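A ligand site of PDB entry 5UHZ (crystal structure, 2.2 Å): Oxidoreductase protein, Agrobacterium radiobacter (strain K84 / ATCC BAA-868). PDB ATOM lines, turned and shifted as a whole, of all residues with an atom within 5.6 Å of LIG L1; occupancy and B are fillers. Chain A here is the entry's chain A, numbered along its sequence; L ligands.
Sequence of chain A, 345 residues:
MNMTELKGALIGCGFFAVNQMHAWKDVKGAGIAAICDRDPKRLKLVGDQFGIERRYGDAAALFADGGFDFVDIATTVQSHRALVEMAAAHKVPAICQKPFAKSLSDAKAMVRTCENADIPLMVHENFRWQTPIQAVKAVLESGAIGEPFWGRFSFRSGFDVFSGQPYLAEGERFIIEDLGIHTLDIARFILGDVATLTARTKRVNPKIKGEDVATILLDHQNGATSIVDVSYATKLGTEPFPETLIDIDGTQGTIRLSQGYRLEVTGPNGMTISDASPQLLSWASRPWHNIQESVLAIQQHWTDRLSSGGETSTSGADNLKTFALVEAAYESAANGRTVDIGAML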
ATOM      1  N   PHE A  15       3.643  -1.259  25.496  1.00  0.00           N
ATOM      2  CA  PHE A  15       4.513  -1.922  24.513  1.00  0.00           C
ATOM      3  C   PHE A  15       4.273  -1.335  23.112  1.00  0.00           C
ATOM      4  O   PHE A  15       5.197  -0.792  22.505  1.00  0.00           O
ATOM      5  CB  PHE A  15       4.300  -3.461  24.596  1.00  0.00           C
ATOM      6  CG  PHE A  15       4.693  -4.235  23.361  1.00  0.00           C
ATOM      7  CD1 PHE A  15       3.731  -4.527  22.380  1.00  0.00           C
ATOM      8  CD2 PHE A  15       5.994  -4.725  23.200  1.00  0.00           C
ATOM      9  CE1 PHE A  15       4.080  -5.264  21.239  1.00  0.00           C
ATOM     10  CE2 PHE A  15       6.331  -5.454  22.064  1.00  0.00           C
ATOM     11  CZ  PHE A  15       5.376  -5.723  21.088  1.00  0.00           C
ATOM     12  N   LYS A  98      -7.657  -1.560  19.355  1.00  0.00           N
ATOM     13  CA  LYS A  98      -8.395  -2.822  19.383  1.00  0.00           C
ATOM     14  C   LYS A  98      -7.911  -3.668  20.568  1.00  0.00           C
ATOM     15  O   LYS A  98      -6.840  -3.391  21.111  1.00  0.00           O
ATOM     16  CB  LYS A  98      -8.311  -3.600  18.060  1.00  0.00           C
ATOM     17  CG  LYS A  98      -6.951  -3.732  17.374  1.00  0.00           C
ATOM     18  CD  LYS A  98      -5.886  -4.490  18.154  1.00  0.00           C
ATOM     19  CE  LYS A  98      -6.286  -5.940  18.447  1.00  0.00           C
ATOM     20  NZ  LYS A  98      -5.105  -6.772  18.816  1.00  0.00           N
ATOM     21  N   PHE A 127      -4.290  -3.441  10.334  1.00  0.00           N
ATOM     22  CA  PHE A 127      -3.964  -4.499   9.353  1.00  0.00           C
ATOM     23  C   PHE A 127      -4.426  -4.173   7.931  1.00  0.00           C
ATOM     24  O   PHE A 127      -3.681  -4.435   6.982  1.00  0.00           O
ATOM     25  CB  PHE A 127      -4.493  -5.863   9.807  1.00  0.00           C
ATOM     26  CG  PHE A 127      -3.540  -6.623  10.707  1.00  0.00           C
ATOM     27  CD1 PHE A 127      -2.998  -6.027  11.836  1.00  0.00           C
ATOM     28  CD2 PHE A 127      -3.185  -7.932  10.419  1.00  0.00           C
ATOM     29  CE1 PHE A 127      -2.114  -6.722  12.661  1.00  0.00           C
ATOM     30  CE2 PHE A 127      -2.312  -8.641  11.239  1.00  0.00           C
ATOM     31  CZ  PHE A 127      -1.770  -8.024  12.355  1.00  0.00           C
ATOM     32  N   VAL A 161       4.330 -14.522  20.503  1.00  0.00           N
ATOM     33  CA  VAL A 161       3.694 -13.221  20.823  1.00  0.00           C
ATOM     34  C   VAL A 161       3.499 -12.977  22.329  1.00  0.00           C
ATOM     35  O   VAL A 161       3.249 -11.847  22.744  1.00  0.00           O
ATOM     36  CB  VAL A 161       2.308 -13.056  20.141  1.00  0.00           C
ATOM     37  CG1 VAL A 161       2.446 -13.120  18.630  1.00  0.00           C
ATOM     38  CG2 VAL A 161       1.295 -14.081  20.659  1.00  0.00           C
ATOM     39  N   GLN A 165       3.522  -9.595  24.879  1.00  0.00           N
ATOM     40  CA  GLN A 165       2.154  -9.358  25.335  1.00  0.00           C
ATOM     41  C   GLN A 165       1.675 -10.497  26.249  1.00  0.00           C
ATOM     42  O   GLN A 165       0.896 -11.348  25.815  1.00  0.00           O
ATOM     43  CB  GLN A 165       1.215  -9.214  24.124  1.00  0.00           C
ATOM     44  CG  GLN A 165       1.481  -7.982  23.276  1.00  0.00           C
ATOM     45  CD  GLN A 165       0.804  -8.031  21.922  1.00  0.00           C
ATOM     46  OE1 GLN A 165       1.450  -8.237  20.901  1.00  0.00           O
ATOM     47  NE2 GLN A 165      -0.517  -7.836  21.894  1.00  0.00           N
ATOM     48  N   TYR A 167      -0.472 -10.835  28.780  1.00  0.00           N
ATOM     49  CA  TYR A 167      -1.953 -10.948  28.897  1.00  0.00           C
ATOM     50  C   TYR A 167      -2.633 -11.919  27.898  1.00  0.00           C
ATOM     51  O   TYR A 167      -3.674 -12.523  28.213  1.00  0.00           O
ATOM     52  CB  TYR A 167      -2.622  -9.547  28.821  1.00  0.00           C
ATOM     53  CG  TYR A 167      -2.294  -8.738  27.573  1.00  0.00           C
ATOM     54  CD1 TYR A 167      -3.026  -8.899  26.390  1.00  0.00           C
ATOM     55  CD2 TYR A 167      -1.259  -7.787  27.586  1.00  0.00           C
ATOM     56  CE1 TYR A 167      -2.717  -8.160  25.248  1.00  0.00           C
ATOM     57  CE2 TYR A 167      -0.948  -7.058  26.444  1.00  0.00           C
ATOM     58  CZ  TYR A 167      -1.683  -7.240  25.288  1.00  0.00           C
ATOM     59  OH  TYR A 167      -1.359  -6.507  24.150  1.00  0.00           O
ATOM     60  N   LEU A 168      -2.033 -12.084  26.716  1.00  0.00           N
ATOM     61  CA  LEU A 168      -2.553 -13.008  25.693  1.00  0.00           C
ATOM     62  C   LEU A 168      -2.622 -14.470  26.154  1.00  0.00           C
ATOM     63  O   LEU A 168      -3.528 -15.201  25.743  1.00  0.00           O
ATOM     64  CB  LEU A 168      -1.720 -12.907  24.392  1.00  0.00           C
ATOM     65  CG  LEU A 168      -1.705 -11.571  23.660  1.00  0.00           C
ATOM     66  CD1 LEU A 168      -0.828 -11.677  22.419  1.00  0.00           C
ATOM     67  CD2 LEU A 168      -3.117 -11.116  23.278  1.00  0.00           C
ATOM     68  N   PHE A 174      -8.619 -15.769  23.405  1.00  0.00           N
ATOM     69  CA  PHE A 174      -7.328 -15.341  22.862  1.00  0.00           C
ATOM     70  C   PHE A 174      -7.389 -15.014  21.364  1.00  0.00           C
ATOM     71  O   PHE A 174      -7.637 -13.852  21.019  1.00  0.00           O
ATOM     72  CB  PHE A 174      -6.233 -16.375  23.217  1.00  0.00           C
ATOM     73  CG  PHE A 174      -4.941 -16.202  22.437  1.00  0.00           C
ATOM     74  CD1 PHE A 174      -4.387 -14.938  22.228  1.00  0.00           C
ATOM     75  CD2 PHE A 174      -4.269 -17.324  21.946  1.00  0.00           C
ATOM     76  CE1 PHE A 174      -3.202 -14.797  21.513  1.00  0.00           C
ATOM     77  CE2 PHE A 174      -3.080 -17.182  21.240  1.00  0.00           C
ATOM     78  CZ  PHE A 174      -2.539 -15.921  21.026  1.00  0.00           C
ATOM     79  N   ASP A 178      -7.857 -11.109  19.718  1.00  0.00           N
ATOM     80  CA  ASP A 178      -6.543 -10.471  19.573  1.00  0.00           C
ATOM     81  C   ASP A 178      -6.152 -10.296  18.104  1.00  0.00           C
ATOM     82  O   ASP A 178      -5.801  -9.191  17.675  1.00  0.00           O
ATOM     83  CB  ASP A 178      -5.461 -11.285  20.285  1.00  0.00           C
ATOM     84  CG  ASP A 178      -4.069 -10.738  20.036  1.00  0.00           C
ATOM     85  OD1 ASP A 178      -3.874  -9.508  20.154  1.00  0.00           O
ATOM     86  OD2 ASP A 178      -3.156 -11.544  19.727  1.00  0.00           O
ATOM     87  N   LEU A 179      -6.169 -11.403  17.355  1.00  0.00           N
ATOM     88  CA  LEU A 179      -5.664 -11.437  15.991  1.00  0.00           C
ATOM     89  C   LEU A 179      -6.771 -11.613  14.952  1.00  0.00           C
ATOM     90  O   LEU A 179      -6.814 -10.872  13.963  1.00  0.00           O
ATOM     91  CB  LEU A 179      -4.650 -12.569  15.829  1.00  0.00           C
ATOM     92  CG  LEU A 179      -4.240 -12.805  14.367  1.00  0.00           C
ATOM     93  CD1 LEU A 179      -3.160 -11.825  13.957  1.00  0.00           C
ATOM     94  CD2 LEU A 179      -3.825 -14.244  14.145  1.00  0.00           C
ATOM     95  N   HIS A 182      -8.410  -8.750  13.335  1.00  0.00           N
ATOM     96  CA  HIS A 182      -7.746  -8.148  12.176  1.00  0.00           C
ATOM     97  C   HIS A 182      -8.112  -8.848  10.854  1.00  0.00           C
ATOM     98  O   HIS A 182      -8.412  -8.201   9.851  1.00  0.00           O
ATOM     99  CB  HIS A 182      -6.228  -8.226  12.297  1.00  0.00           C
ATOM    100  CG  HIS A 182      -5.644  -7.430  13.418  1.00  0.00           C
ATOM    101  ND1 HIS A 182      -5.784  -6.068  13.520  1.00  0.00           N
ATOM    102  CD2 HIS A 182      -4.844  -7.810  14.443  1.00  0.00           C
ATOM    103  CE1 HIS A 182      -5.132  -5.637  14.586  1.00  0.00           C
ATOM    104  NE2 HIS A 182      -4.560  -6.678  15.164  1.00  0.00           N
ATOM    105  N   TYR A 232      -1.989 -19.657  16.185  1.00  0.00           N
ATOM    106  CA  TYR A 232      -0.650 -19.459  16.779  1.00  0.00           C
ATOM    107  C   TYR A 232      -0.016 -20.793  17.241  1.00  0.00           C
ATOM    108  O   TYR A 232       0.873 -20.790  18.091  1.00  0.00           O
ATOM    109  CB  TYR A 232      -0.724 -18.447  17.936  1.00  0.00           C
ATOM    110  CG  TYR A 232      -0.596 -16.999  17.493  1.00  0.00           C
ATOM    111  CD1 TYR A 232       0.549 -16.559  16.828  1.00  0.00           C
ATOM    112  CD2 TYR A 232      -1.598 -16.063  17.772  1.00  0.00           C
ATOM    113  CE1 TYR A 232       0.684 -15.235  16.419  1.00  0.00           C
ATOM    114  CE2 TYR A 232      -1.474 -14.732  17.367  1.00  0.00           C
ATOM    115  CZ  TYR A 232      -0.331 -14.333  16.697  1.00  0.00           C
ATOM    116  OH  TYR A 232      -0.177 -13.045  16.283  1.00  0.00           O
ATOM    117  N   PHE A 241       5.262 -14.837  10.402  1.00  0.00           N
ATOM    118  CA  PHE A 241       4.752 -13.747  11.266  1.00  0.00           C
ATOM    119  C   PHE A 241       5.298 -12.378  10.803  1.00  0.00           C
ATOM    120  O   PHE A 241       6.500 -12.260  10.594  1.00  0.00           O
ATOM    121  CB  PHE A 241       5.144 -14.010  12.724  1.00  0.00           C
ATOM    122  CG  PHE A 241       4.663 -12.965  13.690  1.00  0.00           C
ATOM    123  CD1 PHE A 241       3.392 -13.056  14.261  1.00  0.00           C
ATOM    124  CD2 PHE A 241       5.487 -11.893  14.043  1.00  0.00           C
ATOM    125  CE1 PHE A 241       2.954 -12.092  15.150  1.00  0.00           C
ATOM    126  CE2 PHE A 241       5.047 -10.939  14.946  1.00  0.00           C
ATOM    127  CZ  PHE A 241       3.780 -11.029  15.504  1.00  0.00           C
ATOM    128  N   PRO A 242       4.457 -11.347  10.652  1.00  0.00           N
ATOM    129  CA  PRO A 242       3.020 -11.345  10.901  1.00  0.00           C
ATOM    130  C   PRO A 242       2.290 -11.067   9.588  1.00  0.00           C
ATOM    131  O   PRO A 242       1.558 -10.078   9.468  1.00  0.00           O
ATOM    132  CB  PRO A 242       2.872 -10.195  11.877  1.00  0.00           C
ATOM    133  CG  PRO A 242       3.864  -9.197  11.372  1.00  0.00           C
ATOM    134  CD  PRO A 242       4.992  -9.968  10.726  1.00  0.00           C
ATOM    135  N   TRP A 288       8.396  -6.837  12.537  1.00  0.00           N
ATOM    136  CA  TRP A 288       7.205  -6.006  12.840  1.00  0.00           C
ATOM    137  C   TRP A 288       6.987  -4.848  11.860  1.00  0.00           C
ATOM    138  O   TRP A 288       5.988  -4.126  11.974  1.00  0.00           O
ATOM    139  CB  TRP A 288       7.331  -5.429  14.255  1.00  0.00           C
ATOM    140  CG  TRP A 288       7.387  -6.448  15.316  1.00  0.00           C
ATOM    141  CD1 TRP A 288       8.494  -7.136  15.736  1.00  0.00           C
ATOM    142  CD2 TRP A 288       6.293  -6.928  16.106  1.00  0.00           C
ATOM    143  NE1 TRP A 288       8.151  -8.008  16.733  1.00  0.00           N
ATOM    144  CE2 TRP A 288       6.799  -7.899  16.985  1.00  0.00           C
ATOM    145  CE3 TRP A 288       4.915  -6.615  16.147  1.00  0.00           C
ATOM    146  CZ2 TRP A 288       5.994  -8.579  17.908  1.00  0.00           C
ATOM    147  CZ3 TRP A 288       4.107  -7.286  17.071  1.00  0.00           C
ATOM    148  CH2 TRP A 288       4.654  -8.256  17.941  1.00  0.00           C
ATOM    149  N   ILE A 291       3.525  -4.002  10.135  1.00  0.00           N
ATOM    150  CA  ILE A 291       2.582  -3.475  11.124  1.00  0.00           C
ATOM    151  C   ILE A 291       2.976  -2.036  11.457  1.00  0.00           C
ATOM    152  O   ILE A 291       2.128  -1.134  11.424  1.00  0.00           O
ATOM    153  CB  ILE A 291       2.518  -4.344  12.400  1.00  0.00           C
ATOM    154  CG1 ILE A 291       1.927  -5.725  12.075  1.00  0.00           C
ATOM    155  CG2 ILE A 291       1.709  -3.655  13.496  1.00  0.00           C
ATOM    156  CD1 ILE A 291       2.021  -6.734  13.195  1.00  0.00           C
HETATM  157  O1  LIG L   1      -1.789  -8.008  19.445  1.00  0.00           O
HETATM  158  C1  LIG L   1      -1.690  -8.480  18.100  1.00  0.00           C
HETATM  159  C2  LIG L   1      -1.947  -7.395  17.115  1.00  0.00           C
HETATM  160  O2  LIG L   1      -2.855  -6.584  17.209  1.00  0.00           O
HETATM  161  O3  LIG L   1      -0.987  -7.427  16.037  1.00  0.00           O
HETATM  162  C3  LIG L   1      -0.100  -8.539  16.232  1.00  0.00           C
HETATM  163  C4  LIG L   1      -0.278  -8.923  17.704  1.00  0.00           C
HETATM  164  O4  LIG L   1       0.699  -8.145  18.421  1.00  0.00           O
HETATM  165  C5  LIG L   1       0.004 -10.397  18.004  1.00  0.00           C
HETATM  166  O5  LIG L   1      -1.159 -11.237  17.847  1.00  0.00           O
HETATM  167  P1  LG2 L   2       0.577  -2.915  27.592  1.00  0.00           P
HETATM  168  O1  LG2 L   2       0.120  -3.594  28.863  1.00  0.00           O
HETATM  169  O2  LG2 L   2       2.016  -3.028  27.166  1.00  0.00           O
HETATM  170  O3  LG2 L   2       0.251  -1.356  27.714  1.00  0.00           O
HETATM  171  C1  LG2 L   2      -0.964  -0.827  28.252  1.00  0.00           C
HETATM  172  C2  LG2 L   2      -0.594   0.390  29.078  1.00  0.00           C
HETATM  173  O4  LG2 L   2      -1.770   1.121  29.396  1.00  0.00           O
HETATM  174  C3  LG2 L   2       0.073   0.021  30.398  1.00  0.00           C
HETATM  175  O5  LG2 L   2       1.314   0.717  30.512  1.00  0.00           O
HETATM  176  C4  LG2 L   2      -0.917   0.450  31.486  1.00  0.00           C
HETATM  177  O6  LG2 L   2      -0.277   0.949  32.660  1.00  0.00           O
HETATM  178  C5  LG2 L   2      -1.737   1.516  30.777  1.00  0.00           C
HETATM  179  N1  LG2 L   2      -3.136   1.703  31.208  1.00  0.00           N
HETATM  180  C6  LG2 L   2      -4.112   0.767  31.276  1.00  0.00           C
HETATM  181  N2  LG2 L   2      -5.279   1.333  31.677  1.00  0.00           N
HETATM  182  C7  LG2 L   2      -5.063   2.650  31.863  1.00  0.00           C
HETATM  183  C8  LG2 L   2      -5.854   3.833  32.291  1.00  0.00           C
HETATM  184  N3  LG2 L   2      -7.170   3.733  32.607  1.00  0.00           N
HETATM  185  N4  LG2 L   2      -5.229   5.030  32.346  1.00  0.00           N
HETATM  186  C9  LG2 L   2      -3.914   5.181  32.035  1.00  0.00           C
HETATM  187  N5  LG2 L   2      -3.145   4.138  31.644  1.00  0.00           N
HETATM  188  C10 LG2 L   2      -3.650   2.882  31.541  1.00  0.00           C
HETATM  189  O7  LG2 L   2      -0.398  -3.395  26.406  1.00  0.00           O
HETATM  190  P2  LG2 L   2       0.054  -3.347  24.846  1.00  0.00           P
HETATM  191  O8  LG2 L   2       0.762  -4.637  24.513  1.00  0.00           O
HETATM  192  O9  LG2 L   2       0.732  -2.026  24.594  1.00  0.00           O
HETATM  193  O10 LG2 L   2      -1.356  -3.385  24.088  1.00  0.00           O
HETATM  194  C11 LG2 L   2      -2.311  -2.350  24.289  1.00  0.00           C
HETATM  195  C12 LG2 L   2      -3.400  -2.470  23.247  1.00  0.00           C
HETATM  196  O11 LG2 L   2      -2.820  -2.430  21.938  1.00  0.00           O
HETATM  197  C13 LG2 L   2      -4.171  -3.784  23.364  1.00  0.00           C
HETATM  198  O12 LG2 L   2      -5.580  -3.511  23.390  1.00  0.00           O
HETATM  199  C14 LG2 L   2      -3.769  -4.587  22.128  1.00  0.00           C
HETATM  200  O13 LG2 L   2      -4.858  -5.359  21.607  1.00  0.00           O
HETATM  201  C15 LG2 L   2      -3.319  -3.508  21.145  1.00  0.00           C
HETATM  202  N6  LG2 L   2      -2.294  -3.898  20.147  1.00  0.00           N
HETATM  203  C16 LG2 L   2      -2.519  -3.548  18.867  1.00  0.00           C
HETATM  204  C17 LG2 L   2      -1.626  -3.850  17.842  1.00  0.00           C
HETATM  205  C18 LG2 L   2      -1.948  -3.432  16.432  1.00  0.00           C
HETATM  206  O14 LG2 L   2      -2.479  -2.344  16.240  1.00  0.00           O
HETATM  207  N7  LG2 L   2      -1.662  -4.230  15.406  1.00  0.00           N
HETATM  208  C19 LG2 L   2      -0.449  -4.538  18.173  1.00  0.00           C
HETATM  209  C20 LG2 L   2      -0.221  -4.887  19.507  1.00  0.00           C
HETATM  210  C21 LG2 L   2      -1.167  -4.558  20.487  1.00  0.00           C
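An oxygen (O5) of LIG L1 is in hydrogen-bond range of the side-chain hydroxyl (OH) of Tyr 232 (2.6 Å).
The side-chain amide oxygen (OE1) of Gln 165 lies within hydrogen-bond range of an oxygen (O4) of LIG L1.
A ring nitrogen (NE2) of His 182 lies within hydrogen-bond range of an oxygen (O2) of LIG L1.
The side-chain carboxylate (OD1) of Asp 178 sits at hydrogen-bond distance from an oxygen (O1) of LIG L1 (2.7 Å).
NZ of Lys 98 lies within hydrogen-bond range of O2 of LIG L1.
O of Lys 98 is in hydrogen-bond range of O12 of LG2 L2 (2.6 Å).
The side-chain amino group (NZ) of Lys 98 lies within hydrogen-bond range of an oxygen (O13) of LG2 L2 (3.1 Å).
O8 of LG2 L2 is in hydrogen-bond range of OH of Tyr 167.
An oxygen (O2) of LG2 L2 is in hydrogen-bond range of the backbone NH of Phe 15.
An oxygen (O2) of LIG L1 sits close to a nitrogen (N7) of LG2 L2 (3.2 Å).
The side-chain hydroxyl of Tyr 167 sits at hydrogen-bond distance from the side-chain amide nitrogen of Gln 165 (2.8 Å).
OD1 of Asp 178 lies within salt-bridge range of NZ of Lys 98 (3.3 Å).
Phe 127 touches LIG L1.
Val 161 touches LIG L1.
Trp 288 touches LIG L1 (CZ3 to O4, 3.8 Å).
Hydrophobic or aromatic side chains that line LIG L1: Phe 127, Val 161, His 182, Tyr 232 and Trp 288.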
